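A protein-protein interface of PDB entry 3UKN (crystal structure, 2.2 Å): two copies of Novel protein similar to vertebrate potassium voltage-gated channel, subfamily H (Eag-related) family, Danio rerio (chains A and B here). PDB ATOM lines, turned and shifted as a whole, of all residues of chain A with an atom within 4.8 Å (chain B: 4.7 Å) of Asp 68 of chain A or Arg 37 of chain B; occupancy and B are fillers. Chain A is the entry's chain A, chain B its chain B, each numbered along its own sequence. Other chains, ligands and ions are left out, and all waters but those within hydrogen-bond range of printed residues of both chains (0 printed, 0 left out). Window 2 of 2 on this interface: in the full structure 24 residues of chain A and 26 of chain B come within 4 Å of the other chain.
The side-chain carboxylate (OD2) of Asp 68 of chain A is in salt-bridge range of the guanidinium group (NH2) of Arg 37 of chain B (3.0 Å).
ND1 of His 72 of chain A is in hydrogen-bond range of O of Asp 68 of chain A, at 3.0 Å.
Among the printed residues, merely in contact across the chains: Leu 65 of chain A with Leu 34 of chain B (3.8 Å), Leu 65 of chain A with Arg 37 of chain B (3.8 Å), Leu 65 of chain A with Cys 41 of chain B (3.8 Å), Ile 69 of chain A with Met 38 of chain B (3.8 Å) and His 72 of chain A with Leu 34 of chain B (3.6 Å).
Printed residues of chain A within 4 Å of Arg 37 of chain B: Leu 65 (3.8 Å) and Asp 68 (3.0 Å).
Of the printed residues of chain A, Cys 41 of chain B touches Leu 65.
Of the printed residues of chain A, Leu 34 of chain B touches Leu 65 (3.8 Å) and His 72 (3.6 Å).
Printed residues of chain B within 4 Å of Leu 65 of chain A: Leu 34, Arg 37 and Cys 41.
Of the printed residues of chain B, Ile 69 of chain A touches Met 38.
Printed residues of chain B within 4 Å of His 72 of chain A: Leu 34 (3.6 Å).
The nearest residue of chain B that does not touch Asp 68 of chain A is Leu 34 of chain B (4.1 Å).
The nearest residue of chain A that does not touch Arg 37 of chain B is Glu 64 of chain A (4.2 Å).
The nearest printed residue of chain B that does not touch His 72 of chain A is Arg 37 of chain B (7.3 Å).
Printed residues of chain B that touch a printed residue of chain A: Leu 34, Arg 37, Met 38 and Cys 41.
Hydrophobic or aromatic side chains of chain B within 4 Å of the printed part of chain A: Leu 34 and Met 38.
Of the 9 printed residues of chain A, 4 touch a printed residue of chain B.
Hydrophobic or aromatic side chains of chain A within 4 Å of the printed part of chain B: Leu 65, Ile 69 and His 72.
Among the printed residues, 6 pairs touch across the chains.
Among the printed residues, Asp or Glu carboxylates within 4 Å of a Lys or Arg side-chain nitrogen of the other chain: Asp 68 of chain A with Arg 37 of chain B (3.0 Å).
No position is printed for both chains.
Of the 6 pairs that touch across the chains among the printed residues, none has its exchanged pair printed and touching as well.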
ATOM      1  N   GLU A  64      26.090 -23.195 -22.876  1.00  0.00           N
ATOM      2  CA  GLU A  64      25.151 -23.653 -23.886  1.00  0.00           C
ATOM      3  C   GLU A  64      24.383 -22.463 -24.426  1.00  0.00           C
ATOM      4  O   GLU A  64      24.281 -22.269 -25.634  1.00  0.00           O
ATOM      5  CB  GLU A  64      24.188 -24.696 -23.293  1.00  0.00           C
ATOM      6  N   LEU A  65      23.849 -21.661 -23.515  1.00  0.00           N
ATOM      7  CA  LEU A  65      23.130 -20.449 -23.883  1.00  0.00           C
ATOM      8  C   LEU A  65      24.032 -19.501 -24.677  1.00  0.00           C
ATOM      9  O   LEU A  65      23.629 -19.003 -25.737  1.00  0.00           O
ATOM     10  CB  LEU A  65      22.576 -19.749 -22.639  1.00  0.00           C
ATOM     11  CG  LEU A  65      21.658 -18.577 -22.958  1.00  0.00           C
ATOM     12  CD1 LEU A  65      20.686 -18.964 -24.052  1.00  0.00           C
ATOM     13  CD2 LEU A  65      20.912 -18.133 -21.714  1.00  0.00           C
ATOM     14  N   ARG A  66      25.243 -19.254 -24.171  1.00  0.00           N
ATOM     15  CA  ARG A  66      26.188 -18.358 -24.850  1.00  0.00           C
ATOM     16  C   ARG A  66      26.508 -18.829 -26.276  1.00  0.00           C
ATOM     17  O   ARG A  66      26.579 -18.027 -27.212  1.00  0.00           O
ATOM     18  CB  ARG A  66      27.470 -18.187 -24.026  1.00  0.00           C
ATOM     19  CG  ARG A  66      27.294 -17.297 -22.801  1.00  0.00           C
ATOM     20  CD  ARG A  66      28.491 -17.362 -21.872  1.00  0.00           C
ATOM     21  NE  ARG A  66      29.749 -17.131 -22.568  1.00  0.00           N
ATOM     22  CZ  ARG A  66      30.257 -15.925 -22.840  1.00  0.00           C
ATOM     23  NH1 ARG A  66      29.615 -14.825 -22.466  1.00  0.00           N
ATOM     24  NH2 ARG A  66      31.423 -15.819 -23.481  1.00  0.00           N
ATOM     25  N   ALA A  67      26.679 -20.137 -26.442  1.00  0.00           N
ATOM     26  CA  ALA A  67      26.944 -20.699 -27.760  1.00  0.00           C
ATOM     27  C   ALA A  67      25.745 -20.470 -28.678  1.00  0.00           C
ATOM     28  O   ALA A  67      25.896 -20.107 -29.851  1.00  0.00           O
ATOM     29  CB  ALA A  67      27.239 -22.172 -27.639  1.00  0.00           C
ATOM     30  N   ASP A  68      24.550 -20.679 -28.132  1.00  0.00           N
ATOM     31  CA  ASP A  68      23.326 -20.571 -28.917  1.00  0.00           C
ATOM     32  C   ASP A  68      23.067 -19.150 -29.372  1.00  0.00           C
ATOM     33  O   ASP A  68      22.615 -18.918 -30.488  1.00  0.00           O
ATOM     34  CB  ASP A  68      22.134 -21.116 -28.140  1.00  0.00           C
ATOM     35  CG  ASP A  68      22.135 -22.627 -28.078  1.00  0.00           C
ATOM     36  OD1 ASP A  68      22.649 -23.247 -29.032  1.00  0.00           O
ATOM     37  OD2 ASP A  68      21.639 -23.199 -27.084  1.00  0.00           O
ATOM     38  N   ILE A  69      23.343 -18.198 -28.495  1.00  0.00           N
ATOM     39  CA  ILE A  69      23.223 -16.797 -28.837  1.00  0.00           C
ATOM     40  C   ILE A  69      24.252 -16.429 -29.903  1.00  0.00           C
ATOM     41  O   ILE A  69      23.932 -15.755 -30.894  1.00  0.00           O
ATOM     42  CB  ILE A  69      23.489 -15.934 -27.604  1.00  0.00           C
ATOM     43  CG1 ILE A  69      22.296 -16.000 -26.641  1.00  0.00           C
ATOM     44  CG2 ILE A  69      23.812 -14.516 -28.021  1.00  0.00           C
ATOM     45  CD1 ILE A  69      22.639 -15.578 -25.245  1.00  0.00           C
ATOM     46  N   ALA A  70      25.492 -16.870 -29.691  1.00  0.00           N
ATOM     47  CA  ALA A  70      26.588 -16.514 -30.585  1.00  0.00           C
ATOM     48  C   ALA A  70      26.363 -17.066 -31.999  1.00  0.00           C
ATOM     49  O   ALA A  70      26.615 -16.378 -32.994  1.00  0.00           O
ATOM     50  CB  ALA A  70      27.939 -16.973 -30.022  1.00  0.00           C
ATOM     51  N   MET A  71      25.871 -18.298 -32.091  1.00  0.00           N
ATOM     52  CA  MET A  71      25.676 -18.884 -33.406  1.00  0.00           C
ATOM     53  C   MET A  71      24.521 -18.221 -34.150  1.00  0.00           C
ATOM     54  O   MET A  71      24.260 -18.545 -35.303  1.00  0.00           O
ATOM     55  CB  MET A  71      25.548 -20.410 -33.345  1.00  0.00           C
ATOM     56  CG  MET A  71      24.146 -20.927 -33.166  1.00  0.00           C
ATOM     57  SD  MET A  71      24.134 -22.724 -33.054  1.00  0.00           S
ATOM     58  CE  MET A  71      25.090 -22.988 -31.554  1.00  0.00           C
ATOM     59  N   HIS A  72      23.865 -17.260 -33.501  1.00  0.00           N
ATOM     60  CA  HIS A  72      22.872 -16.411 -34.161  1.00  0.00           C
ATOM     61  C   HIS A  72      23.460 -15.065 -34.614  1.00  0.00           C
ATOM     62  O   HIS A  72      22.765 -14.251 -35.226  1.00  0.00           O
ATOM     63  CB  HIS A  72      21.682 -16.150 -33.238  1.00  0.00           C
ATOM     64  CG  HIS A  72      20.593 -17.172 -33.345  1.00  0.00           C
ATOM     65  ND1 HIS A  72      20.632 -18.379 -32.679  1.00  0.00           N
ATOM     66  CD2 HIS A  72      19.437 -17.167 -34.052  1.00  0.00           C
ATOM     67  CE1 HIS A  72      19.546 -19.073 -32.969  1.00  0.00           C
ATOM     68  NE2 HIS A  72      18.805 -18.360 -33.799  1.00  0.00           N
ATOM     69  N   ALA B  33      11.917 -18.437 -28.424  1.00  0.00           N
ATOM     70  CA  ALA B  33      12.369 -19.373 -27.397  1.00  0.00           C
ATOM     71  C   ALA B  33      13.737 -18.965 -26.837  1.00  0.00           C
ATOM     72  O   ALA B  33      13.962 -19.003 -25.631  1.00  0.00           O
ATOM     73  CB  ALA B  33      12.397 -20.803 -27.934  1.00  0.00           C
ATOM     74  N   LEU B  34      14.647 -18.570 -27.718  1.00  0.00           N
ATOM     75  CA  LEU B  34      15.989 -18.189 -27.302  1.00  0.00           C
ATOM     76  C   LEU B  34      15.901 -16.982 -26.365  1.00  0.00           C
ATOM     77  O   LEU B  34      16.449 -16.996 -25.256  1.00  0.00           O
ATOM     78  CB  LEU B  34      16.867 -17.894 -28.526  1.00  0.00           C
ATOM     79  CG  LEU B  34      18.311 -17.389 -28.328  1.00  0.00           C
ATOM     80  CD1 LEU B  34      19.161 -18.354 -27.499  1.00  0.00           C
ATOM     81  CD2 LEU B  34      18.952 -17.151 -29.698  1.00  0.00           C
ATOM     82  N   ALA B  35      15.184 -15.956 -26.809  1.00  0.00           N
ATOM     83  CA  ALA B  35      14.913 -14.783 -25.984  1.00  0.00           C
ATOM     84  C   ALA B  35      14.383 -15.176 -24.609  1.00  0.00           C
ATOM     85  O   ALA B  35      14.879 -14.708 -23.588  1.00  0.00           O
ATOM     86  CB  ALA B  35      13.921 -13.872 -26.686  1.00  0.00           C
ATOM     87  N   GLN B  36      13.365 -16.032 -24.585  1.00  0.00           N
ATOM     88  CA  GLN B  36      12.812 -16.518 -23.322  1.00  0.00           C
ATOM     89  C   GLN B  36      13.917 -17.108 -22.433  1.00  0.00           C
ATOM     90  O   GLN B  36      14.012 -16.775 -21.265  1.00  0.00           O
ATOM     91  CB  GLN B  36      11.705 -17.557 -23.570  1.00  0.00           C
ATOM     92  CG  GLN B  36      10.308 -17.106 -23.157  1.00  0.00           C
ATOM     93  CD  GLN B  36       9.200 -17.996 -23.727  1.00  0.00           C
ATOM     94  OE1 GLN B  36       9.165 -18.286 -24.932  1.00  0.00           O
ATOM     95  NE2 GLN B  36       8.292 -18.433 -22.859  1.00  0.00           N
ATOM     96  N   ARG B  37      14.751 -17.982 -22.995  1.00  0.00           N
ATOM     97  CA  ARG B  37      15.860 -18.557 -22.237  1.00  0.00           C
ATOM     98  C   ARG B  37      16.732 -17.471 -21.608  1.00  0.00           C
ATOM     99  O   ARG B  37      17.166 -17.606 -20.456  1.00  0.00           O
ATOM    100  CB  ARG B  37      16.724 -19.447 -23.124  1.00  0.00           C
ATOM    101  CG  ARG B  37      16.010 -20.661 -23.656  1.00  0.00           C
ATOM    102  CD  ARG B  37      16.817 -21.313 -24.761  1.00  0.00           C
ATOM    103  NE  ARG B  37      18.084 -21.843 -24.271  1.00  0.00           N
ATOM    104  CZ  ARG B  37      19.067 -22.254 -25.061  1.00  0.00           C
ATOM    105  NH1 ARG B  37      18.930 -22.183 -26.377  1.00  0.00           N
ATOM    106  NH2 ARG B  37      20.188 -22.728 -24.539  1.00  0.00           N
ATOM    107  N   MET B  38      16.973 -16.404 -22.365  1.00  0.00           N
ATOM    108  CA  MET B  38      17.864 -15.323 -21.944  1.00  0.00           C
ATOM    109  C   MET B  38      17.290 -14.494 -20.805  1.00  0.00           C
ATOM    110  O   MET B  38      18.009 -14.134 -19.875  1.00  0.00           O
ATOM    111  CB  MET B  38      18.214 -14.414 -23.134  1.00  0.00           C
ATOM    112  CG  MET B  38      18.987 -15.115 -24.250  1.00  0.00           C
ATOM    113  SD  MET B  38      19.138 -14.140 -25.769  1.00  0.00           S
ATOM    114  CE  MET B  38      20.071 -12.725 -25.225  1.00  0.00           C
ATOM    115  N   LEU B  39      15.997 -14.188 -20.888  1.00  0.00           N
ATOM    116  CA  LEU B  39      15.330 -13.369 -19.876  1.00  0.00           C
ATOM    117  C   LEU B  39      15.194 -14.078 -18.528  1.00  0.00           C
ATOM    118  O   LEU B  39      15.294 -13.446 -17.473  1.00  0.00           O
ATOM    119  CB  LEU B  39      13.963 -12.891 -20.377  1.00  0.00           C
ATOM    120  CG  LEU B  39      14.026 -11.985 -21.617  1.00  0.00           C
ATOM    121  CD1 LEU B  39      12.660 -11.407 -21.962  1.00  0.00           C
ATOM    122  CD2 LEU B  39      15.069 -10.856 -21.438  1.00  0.00           C
ATOM    123  N   GLU B  40      14.962 -15.388 -18.560  1.00  0.00           N
ATOM    124  CA  GLU B  40      14.867 -16.150 -17.321  1.00  0.00           C
ATOM    125  C   GLU B  40      16.253 -16.504 -16.777  1.00  0.00           C
ATOM    126  O   GLU B  40      16.439 -16.619 -15.572  1.00  0.00           O
ATOM    127  CB  GLU B  40      13.951 -17.385 -17.464  1.00  0.00           C
ATOM    128  CG  GLU B  40      14.213 -18.285 -18.664  1.00  0.00           C
ATOM    129  CD  GLU B  40      13.022 -19.200 -19.008  1.00  0.00           C
ATOM    130  OE1 GLU B  40      13.181 -20.074 -19.889  1.00  0.00           O
ATOM    131  OE2 GLU B  40      11.930 -19.042 -18.410  1.00  0.00           O
ATOM    132  N   CYS B  41      17.232 -16.655 -17.662  1.00  0.00           N
ATOM    133  CA  CYS B  41      18.602 -16.840 -17.198  1.00  0.00           C
ATOM    134  C   CYS B  41      19.156 -15.524 -16.626  1.00  0.00           C
ATOM    135  O   CYS B  41      19.848 -15.521 -15.605  1.00  0.00           O
ATOM    136  CB  CYS B  41      19.498 -17.398 -18.300  1.00  0.00           C
ATOM    137  SG  CYS B  41      21.224 -17.583 -17.802  1.00  0.00           S
